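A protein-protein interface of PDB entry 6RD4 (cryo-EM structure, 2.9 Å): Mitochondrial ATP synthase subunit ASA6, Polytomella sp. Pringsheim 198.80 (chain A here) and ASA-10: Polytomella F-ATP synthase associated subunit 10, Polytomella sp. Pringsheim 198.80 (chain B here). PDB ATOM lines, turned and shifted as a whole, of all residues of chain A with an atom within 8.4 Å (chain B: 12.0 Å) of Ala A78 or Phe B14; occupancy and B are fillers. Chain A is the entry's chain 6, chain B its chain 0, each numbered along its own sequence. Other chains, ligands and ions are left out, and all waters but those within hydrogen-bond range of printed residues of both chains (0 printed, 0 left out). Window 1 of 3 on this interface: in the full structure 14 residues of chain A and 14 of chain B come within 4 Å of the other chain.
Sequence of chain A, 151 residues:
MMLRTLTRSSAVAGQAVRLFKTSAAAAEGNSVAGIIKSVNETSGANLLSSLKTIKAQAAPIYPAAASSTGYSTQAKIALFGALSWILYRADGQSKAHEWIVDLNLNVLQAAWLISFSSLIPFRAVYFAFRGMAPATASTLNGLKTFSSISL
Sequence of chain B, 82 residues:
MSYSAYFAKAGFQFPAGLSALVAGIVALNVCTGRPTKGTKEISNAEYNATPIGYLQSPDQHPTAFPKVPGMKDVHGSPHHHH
Ser A72 touches Gly B11 (OG to CA, 3.9 Å).
OG of Ser A72 touches N of Phe B12, at 3.8 Å.
CD2 of Phe B12 touches O of Gln A74, at 3.5 Å.
Gln A74 touches Gln B13 (NE2 to CA, 3.4 Å).
Ala A75 touches Phe B12 (CB to CB, 3.7 Å).
Phe B12 touches Ala A78 (CE2 to CB, 3.7 Å).
CE1 of Phe B14 touches CB of Ala A78, at 3.8 Å.
Printed residues of chain B within 4 Å of Ala A78: Phe B12 and Phe B14.
Printed residues of chain A within 4 Å of Phe B14: Gln A74 and Ala A78.
Gln A74 touches just these residues of chain B: Phe B12 (3.5 Å), Gln B13 (3.4 Å) and Phe B14 (3.0 Å).
Ala A75 touches just one residue of chain B: Phe B12 (3.7 Å).
No residue of chain B comes within 4 Å of Ile A77.
No residue of chain B comes within 4 Å of Leu A79.
No residue of chain B comes within 4 Å of Ala A82.
Pro B15 touches none of the printed residues of chain A.
Of the printed residues of chain A, Gln B13 touches Gln A74.
Of the printed residues of chain B, Ser A72 touches Gly B11 and Phe B12.
Printed residues of chain A within 4 Å of Phe B12: Ser A72 (3.8 Å), Gln A74 (3.5 Å), Ala A75 (3.7 Å) and Ala A78 (3.7 Å).
Of the printed residues of chain A, Gly B11 touches Ser A72 (3.9 Å).
The nearest residue of chain A that does not touch Phe B14 is Ile A77 (4.1 Å).
Printed residues of chain A that touch a printed residue of chain B: Ser A72, Gln A74, Ala A75 and Ala A78.
Hydrophobic or aromatic side chains of chain A that line the printed part of chain B: Ala A75 and Ala A78.
Printed residues of chain B that touch a printed residue of chain A: Gly B11, Phe B12, Gln B13 and Phe B14.
Hydrophobic or aromatic side chains of chain B that line the printed part of chain A: Phe B12 and Phe B14.
NE2 of Gln A74 lies close to N of Phe B14 (3.0 Å).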
ATOM      1  N   SER A  72     -21.079 -10.485  -9.791  1.00  0.00           N
ATOM      2  CA  SER A  72     -22.323 -11.238  -9.723  1.00  0.00           C
ATOM      3  C   SER A  72     -23.524 -10.542 -10.339  1.00  0.00           C
ATOM      4  O   SER A  72     -23.506  -9.330 -10.559  1.00  0.00           O
ATOM      5  CB  SER A  72     -22.646 -11.505  -8.260  1.00  0.00           C
ATOM      6  OG  SER A  72     -21.561 -12.138  -7.629  1.00  0.00           O
ATOM      7  N   THR A  73     -24.598 -11.290 -10.577  1.00  0.00           N
ATOM      8  CA  THR A  73     -25.831 -10.694 -11.073  1.00  0.00           C
ATOM      9  C   THR A  73     -26.467  -9.719 -10.102  1.00  0.00           C
ATOM     10  O   THR A  73     -27.345  -8.965 -10.510  1.00  0.00           O
ATOM     11  CB  THR A  73     -26.846 -11.775 -11.408  1.00  0.00           C
ATOM     12  OG1 THR A  73     -28.084 -11.158 -11.783  1.00  0.00           O
ATOM     13  CG2 THR A  73     -27.071 -12.683 -10.223  1.00  0.00           C
ATOM     14  N   GLN A  74     -26.074  -9.733  -8.834  1.00  0.00           N
ATOM     15  CA  GLN A  74     -26.508  -8.743  -7.868  1.00  0.00           C
ATOM     16  C   GLN A  74     -25.472  -7.676  -7.593  1.00  0.00           C
ATOM     17  O   GLN A  74     -25.816  -6.648  -7.027  1.00  0.00           O
ATOM     18  CB  GLN A  74     -26.880  -9.418  -6.560  1.00  0.00           C
ATOM     19  CG  GLN A  74     -27.992 -10.394  -6.708  1.00  0.00           C
ATOM     20  CD  GLN A  74     -28.393 -10.998  -5.407  1.00  0.00           C
ATOM     21  OE1 GLN A  74     -29.116 -11.978  -5.367  1.00  0.00           O
ATOM     22  NE2 GLN A  74     -27.897 -10.444  -4.329  1.00  0.00           N
ATOM     23  N   ALA A  75     -24.216  -7.896  -7.939  1.00  0.00           N
ATOM     24  CA  ALA A  75     -23.267  -6.800  -7.854  1.00  0.00           C
ATOM     25  C   ALA A  75     -23.400  -5.869  -9.032  1.00  0.00           C
ATOM     26  O   ALA A  75     -22.914  -4.741  -8.984  1.00  0.00           O
ATOM     27  CB  ALA A  75     -21.844  -7.319  -7.784  1.00  0.00           C
ATOM     28  N   LYS A  76     -24.017  -6.328 -10.110  1.00  0.00           N
ATOM     29  CA  LYS A  76     -24.298  -5.434 -11.212  1.00  0.00           C
ATOM     30  C   LYS A  76     -25.560  -4.636 -10.968  1.00  0.00           C
ATOM     31  O   LYS A  76     -25.631  -3.479 -11.376  1.00  0.00           O
ATOM     32  CB  LYS A  76     -24.392  -6.229 -12.506  1.00  0.00           C
ATOM     33  CG  LYS A  76     -23.077  -6.878 -12.907  1.00  0.00           C
ATOM     34  CD  LYS A  76     -23.207  -7.674 -14.190  1.00  0.00           C
ATOM     35  CE  LYS A  76     -24.349  -8.665 -14.115  1.00  0.00           C
ATOM     36  NZ  LYS A  76     -24.362  -9.637 -15.231  1.00  0.00           N
ATOM     37  N   ILE A  77     -26.550  -5.216 -10.292  1.00  0.00           N
ATOM     38  CA  ILE A  77     -27.720  -4.450  -9.877  1.00  0.00           C
ATOM     39  C   ILE A  77     -27.330  -3.414  -8.836  1.00  0.00           C
ATOM     40  O   ILE A  77     -27.854  -2.300  -8.820  1.00  0.00           O
ATOM     41  CB  ILE A  77     -28.813  -5.398  -9.360  1.00  0.00           C
ATOM     42  CG1 ILE A  77     -29.276  -6.310 -10.470  1.00  0.00           C
ATOM     43  CG2 ILE A  77     -30.002  -4.654  -8.870  1.00  0.00           C
ATOM     44  CD1 ILE A  77     -30.212  -7.372 -10.007  1.00  0.00           C
ATOM     45  N   ALA A  78     -26.371  -3.741  -7.986  1.00  0.00           N
ATOM     46  CA  ALA A  78     -25.977  -2.812  -6.946  1.00  0.00           C
ATOM     47  C   ALA A  78     -25.171  -1.653  -7.494  1.00  0.00           C
ATOM     48  O   ALA A  78     -25.164  -0.583  -6.893  1.00  0.00           O
ATOM     49  CB  ALA A  78     -25.178  -3.532  -5.874  1.00  0.00           C
ATOM     50  N   LEU A  79     -24.469  -1.839  -8.604  1.00  0.00           N
ATOM     51  CA  LEU A  79     -23.694  -0.746  -9.172  1.00  0.00           C
ATOM     52  C   LEU A  79     -24.409  -0.033 -10.296  1.00  0.00           C
ATOM     53  O   LEU A  79     -24.152   1.148 -10.523  1.00  0.00           O
ATOM     54  CB  LEU A  79     -22.341  -1.234  -9.680  1.00  0.00           C
ATOM     55  CG  LEU A  79     -21.386  -1.762  -8.626  1.00  0.00           C
ATOM     56  CD1 LEU A  79     -20.361  -2.668  -9.263  1.00  0.00           C
ATOM     57  CD2 LEU A  79     -20.715  -0.604  -7.943  1.00  0.00           C
ATOM     58  N   PHE A  80     -25.277  -0.713 -11.034  1.00  0.00           N
ATOM     59  CA  PHE A  80     -26.099   0.037 -11.964  1.00  0.00           C
ATOM     60  C   PHE A  80     -27.196   0.774 -11.234  1.00  0.00           C
ATOM     61  O   PHE A  80     -27.520   1.901 -11.598  1.00  0.00           O
ATOM     62  CB  PHE A  80     -26.707  -0.862 -13.030  1.00  0.00           C
ATOM     63  CG  PHE A  80     -27.598  -0.132 -13.987  1.00  0.00           C
ATOM     64  CD1 PHE A  80     -28.967  -0.359 -14.000  1.00  0.00           C
ATOM     65  CD2 PHE A  80     -27.071   0.795 -14.868  1.00  0.00           C
ATOM     66  CE1 PHE A  80     -29.790   0.323 -14.887  1.00  0.00           C
ATOM     67  CE2 PHE A  80     -27.887   1.480 -15.755  1.00  0.00           C
ATOM     68  CZ  PHE A  80     -29.247   1.240 -15.766  1.00  0.00           C
ATOM     69  N   GLY A  81     -27.761   0.168 -10.194  1.00  0.00           N
ATOM     70  CA  GLY A  81     -28.774   0.843  -9.408  1.00  0.00           C
ATOM     71  C   GLY A  81     -28.233   1.976  -8.567  1.00  0.00           C
ATOM     72  O   GLY A  81     -28.977   2.881  -8.203  1.00  0.00           O
ATOM     73  N   ALA A  82     -26.953   1.938  -8.226  1.00  0.00           N
ATOM     74  CA  ALA A  82     -26.351   3.076  -7.551  1.00  0.00           C
ATOM     75  C   ALA A  82     -25.950   4.153  -8.527  1.00  0.00           C
ATOM     76  O   ALA A  82     -25.907   5.324  -8.161  1.00  0.00           O
ATOM     77  CB  ALA A  82     -25.130   2.657  -6.754  1.00  0.00           C
ATOM     78  N   LEU A  83     -25.607   3.778  -9.753  1.00  0.00           N
ATOM     79  CA  LEU A  83     -25.356   4.774 -10.783  1.00  0.00           C
ATOM     80  C   LEU A  83     -26.657   5.352 -11.293  1.00  0.00           C
ATOM     81  O   LEU A  83     -26.725   6.529 -11.640  1.00  0.00           O
ATOM     82  CB  LEU A  83     -24.573   4.155 -11.927  1.00  0.00           C
ATOM     83  CG  LEU A  83     -24.058   5.103 -12.991  1.00  0.00           C
ATOM     84  CD1 LEU A  83     -22.831   5.829 -12.483  1.00  0.00           C
ATOM     85  CD2 LEU A  83     -23.778   4.344 -14.263  1.00  0.00           C
ATOM     86  N   SER A  84     -27.709   4.544 -11.336  1.00  0.00           N
ATOM     87  CA  SER A  84     -29.022   5.061 -11.686  1.00  0.00           C
ATOM     88  C   SER A  84     -29.590   5.948 -10.597  1.00  0.00           C
ATOM     89  O   SER A  84     -30.519   6.711 -10.853  1.00  0.00           O
ATOM     90  CB  SER A  84     -29.979   3.918 -11.968  1.00  0.00           C
ATOM     91  OG  SER A  84     -31.287   4.405 -12.114  1.00  0.00           O
ATOM     92  N   TRP A  85     -29.091   5.829  -9.372  1.00  0.00           N
ATOM     93  CA  TRP A  85     -29.516   6.710  -8.296  1.00  0.00           C
ATOM     94  C   TRP A  85     -28.688   7.975  -8.269  1.00  0.00           C
ATOM     95  O   TRP A  85     -29.221   9.052  -8.026  1.00  0.00           O
ATOM     96  CB  TRP A  85     -29.416   5.990  -6.959  1.00  0.00           C
ATOM     97  CG  TRP A  85     -29.762   6.820  -5.796  1.00  0.00           C
ATOM     98  CD1 TRP A  85     -28.910   7.375  -4.914  1.00  0.00           C
ATOM     99  CD2 TRP A  85     -31.067   7.176  -5.374  1.00  0.00           C
ATOM    100  NE1 TRP A  85     -29.597   8.071  -3.971  1.00  0.00           N
ATOM    101  CE2 TRP A  85     -30.932   7.962  -4.234  1.00  0.00           C
ATOM    102  CE3 TRP A  85     -32.342   6.909  -5.855  1.00  0.00           C
ATOM    103  CZ2 TRP A  85     -32.017   8.483  -3.571  1.00  0.00           C
ATOM    104  CZ3 TRP A  85     -33.410   7.430  -5.198  1.00  0.00           C
ATOM    105  CH2 TRP A  85     -33.246   8.203  -4.071  1.00  0.00           C
ATOM    106  N   ALA B  10     -18.822 -17.093  -3.256  1.00  0.00           N
ATOM    107  CA  ALA B  10     -20.051 -16.318  -3.262  1.00  0.00           C
ATOM    108  C   ALA B  10     -19.685 -14.849  -3.215  1.00  0.00           C
ATOM    109  O   ALA B  10     -18.999 -14.405  -2.293  1.00  0.00           O
ATOM    110  CB  ALA B  10     -20.936 -16.701  -2.084  1.00  0.00           C
ATOM    111  N   GLY B  11     -20.098 -14.101  -4.223  1.00  0.00           N
ATOM    112  CA  GLY B  11     -19.645 -12.737  -4.332  1.00  0.00           C
ATOM    113  C   GLY B  11     -20.477 -11.780  -3.518  1.00  0.00           C
ATOM    114  O   GLY B  11     -20.724 -12.018  -2.338  1.00  0.00           O
ATOM    115  N   PHE B  12     -20.894 -10.685  -4.133  1.00  0.00           N
ATOM    116  CA  PHE B  12     -21.819  -9.775  -3.491  1.00  0.00           C
ATOM    117  C   PHE B  12     -23.184 -10.422  -3.377  1.00  0.00           C
ATOM    118  O   PHE B  12     -23.575 -11.250  -4.195  1.00  0.00           O
ATOM    119  CB  PHE B  12     -21.925  -8.483  -4.283  1.00  0.00           C
ATOM    120  CG  PHE B  12     -22.751  -7.425  -3.630  1.00  0.00           C
ATOM    121  CD1 PHE B  12     -22.209  -6.613  -2.674  1.00  0.00           C
ATOM    122  CD2 PHE B  12     -24.059  -7.227  -4.001  1.00  0.00           C
ATOM    123  CE1 PHE B  12     -22.963  -5.646  -2.094  1.00  0.00           C
ATOM    124  CE2 PHE B  12     -24.806  -6.267  -3.419  1.00  0.00           C
ATOM    125  CZ  PHE B  12     -24.265  -5.479  -2.468  1.00  0.00           C
ATOM    126  N   GLN B  13     -23.899 -10.047  -2.331  1.00  0.00           N
ATOM    127  CA  GLN B  13     -25.261 -10.488  -2.127  1.00  0.00           C
ATOM    128  C   GLN B  13     -25.960  -9.403  -1.334  1.00  0.00           C
ATOM    129  O   GLN B  13     -25.358  -8.793  -0.452  1.00  0.00           O
ATOM    130  CB  GLN B  13     -25.288 -11.817  -1.395  1.00  0.00           C
ATOM    131  CG  GLN B  13     -26.345 -12.748  -1.855  1.00  0.00           C
ATOM    132  CD  GLN B  13     -26.093 -14.128  -1.355  1.00  0.00           C
ATOM    133  OE1 GLN B  13     -25.000 -14.432  -0.892  1.00  0.00           O
ATOM    134  NE2 GLN B  13     -27.108 -14.975  -1.415  1.00  0.00           N
ATOM    135  N   PHE B  14     -27.218  -9.156  -1.657  1.00  0.00           N
ATOM    136  CA  PHE B  14     -27.980  -8.142  -0.970  1.00  0.00           C
ATOM    137  C   PHE B  14     -28.324  -8.630   0.430  1.00  0.00           C
ATOM    138  O   PHE B  14     -28.161  -9.811   0.731  1.00  0.00           O
ATOM    139  CB  PHE B  14     -29.246  -7.832  -1.751  1.00  0.00           C
ATOM    140  CG  PHE B  14     -29.025  -6.947  -2.919  1.00  0.00           C
ATOM    141  CD1 PHE B  14     -28.283  -5.800  -2.798  1.00  0.00           C
ATOM    142  CD2 PHE B  14     -29.567  -7.255  -4.142  1.00  0.00           C
ATOM    143  CE1 PHE B  14     -28.084  -4.990  -3.877  1.00  0.00           C
ATOM    144  CE2 PHE B  14     -29.363  -6.445  -5.216  1.00  0.00           C
ATOM    145  CZ  PHE B  14     -28.625  -5.316  -5.080  1.00  0.00           C
ATOM    146  N   PRO B  15     -28.766  -7.741   1.319  1.00  0.00           N
ATOM    147  CA  PRO B  15     -29.333  -8.206   2.575  1.00  0.00           C
ATOM    148  C   PRO B  15     -30.558  -9.062   2.338  1.00  0.00           C
ATOM    149  O   PRO B  15     -31.241  -8.962   1.324  1.00  0.00           O
ATOM    150  CB  PRO B  15     -29.670  -6.916   3.296  1.00  0.00           C
ATOM    151  CG  PRO B  15     -28.635  -6.048   2.873  1.00  0.00           C
ATOM    152  CD  PRO B  15     -28.394  -6.329   1.437  1.00  0.00           C
ATOM    153  N   ALA B  16     -30.813  -9.941   3.287  1.00  0.00           N
ATOM    154  CA  ALA B  16     -31.639 -11.100   3.025  1.00  0.00           C
ATOM    155  C   ALA B  16     -33.120 -10.824   2.996  1.00  0.00           C
ATOM    156  O   ALA B  16     -33.888 -11.768   3.132  1.00  0.00           O
ATOM    157  CB  ALA B  16     -31.367 -12.162   4.060  1.00  0.00           C
ATOM    158  N   GLY B  17     -33.554  -9.589   2.900  1.00  0.00           N
ATOM    159  CA  GLY B  17     -34.946  -9.372   2.605  1.00  0.00           C
ATOM    160  C   GLY B  17     -35.159  -8.052   1.929  1.00  0.00           C
ATOM    161  O   GLY B  17     -36.235  -7.476   2.051  1.00  0.00           O
ATOM    162  N   LEU B  18     -34.147  -7.573   1.211  1.00  0.00           N
ATOM    163  CA  LEU B  18     -34.136  -6.208   0.711  1.00  0.00           C
ATOM    164  C   LEU B  18     -35.187  -5.968  -0.344  1.00  0.00           C
ATOM    165  O   LEU B  18     -35.583  -4.828  -0.561  1.00  0.00           O
ATOM    166  CB  LEU B  18     -32.777  -5.872   0.135  1.00  0.00           C
ATOM    167  CG  LEU B  18     -32.426  -4.404   0.065  1.00  0.00           C
ATOM    168  CD1 LEU B  18     -32.372  -3.835   1.436  1.00  0.00           C
ATOM    169  CD2 LEU B  18     -31.118  -4.241  -0.621  1.00  0.00           C
ATOM    170  N   SER B  19     -35.661  -7.015  -0.986  1.00  0.00           N
ATOM    171  CA  SER B  19     -36.723  -6.857  -1.951  1.00  0.00           C
ATOM    172  C   SER B  19     -38.040  -6.507  -1.287  1.00  0.00           C
ATOM    173  O   SER B  19     -38.932  -6.001  -1.954  1.00  0.00           O
ATOM    174  CB  SER B  19     -36.841  -8.128  -2.771  1.00  0.00           C
ATOM    175  OG  SER B  19     -37.109  -9.232  -1.935  1.00  0.00           O
ATOM    176  N   ALA B  20     -38.197  -6.771   0.004  1.00  0.00           N
ATOM    177  CA  ALA B  20     -39.391  -6.328   0.704  1.00  0.00           C
ATOM    178  C   ALA B  20     -39.252  -4.925   1.262  1.00  0.00           C
ATOM    179  O   ALA B  20     -40.256  -4.320   1.634  1.00  0.00           O
ATOM    180  CB  ALA B  20     -39.736  -7.282   1.834  1.00  0.00           C
ATOM    181  N   LEU B  21     -38.038  -4.408   1.372  1.00  0.00           N
ATOM    182  CA  LEU B  21     -37.876  -3.011   1.731  1.00  0.00           C
ATOM    183  C   LEU B  21     -38.083  -2.126   0.520  1.00  0.00           C
ATOM    184  O   LEU B  21     -38.756  -1.103   0.607  1.00  0.00           O
ATOM    185  CB  LEU B  21     -36.496  -2.778   2.322  1.00  0.00           C
ATOM    186  CG  LEU B  21     -36.223  -1.382   2.842  1.00  0.00           C
ATOM    187  CD1 LEU B  21     -37.155  -1.106   3.944  1.00  0.00           C
ATOM    188  CD2 LEU B  21     -34.824  -1.259   3.321  1.00  0.00           C
ATOM    189  N   VAL B  22     -37.522  -2.516  -0.617  1.00  0.00           N
ATOM    190  CA  VAL B  22     -37.651  -1.730  -1.831  1.00  0.00           C
ATOM    191  C   VAL B  22     -39.067  -1.821  -2.374  1.00  0.00           C
ATOM    192  O   VAL B  22     -39.595  -0.853  -2.911  1.00  0.00           O
ATOM    193  CB  VAL B  22     -36.592  -2.189  -2.844  1.00  0.00           C
ATOM    194  CG1 VAL B  22     -36.679  -1.419  -4.120  1.00  0.00           C
ATOM    195  CG2 VAL B  22     -35.227  -2.005  -2.252  1.00  0.00           C
ATOM    196  N   ALA B  23     -39.730  -2.953  -2.203  1.00  0.00           N
ATOM    197  CA  ALA B  23     -41.126  -3.009  -2.613  1.00  0.00           C
ATOM    198  C   ALA B  23     -42.039  -2.368  -1.595  1.00  0.00           C
ATOM    199  O   ALA B  23     -43.227  -2.215  -1.858  1.00  0.00           O
ATOM    200  CB  ALA B  23     -41.586  -4.437  -2.852  1.00  0.00           C
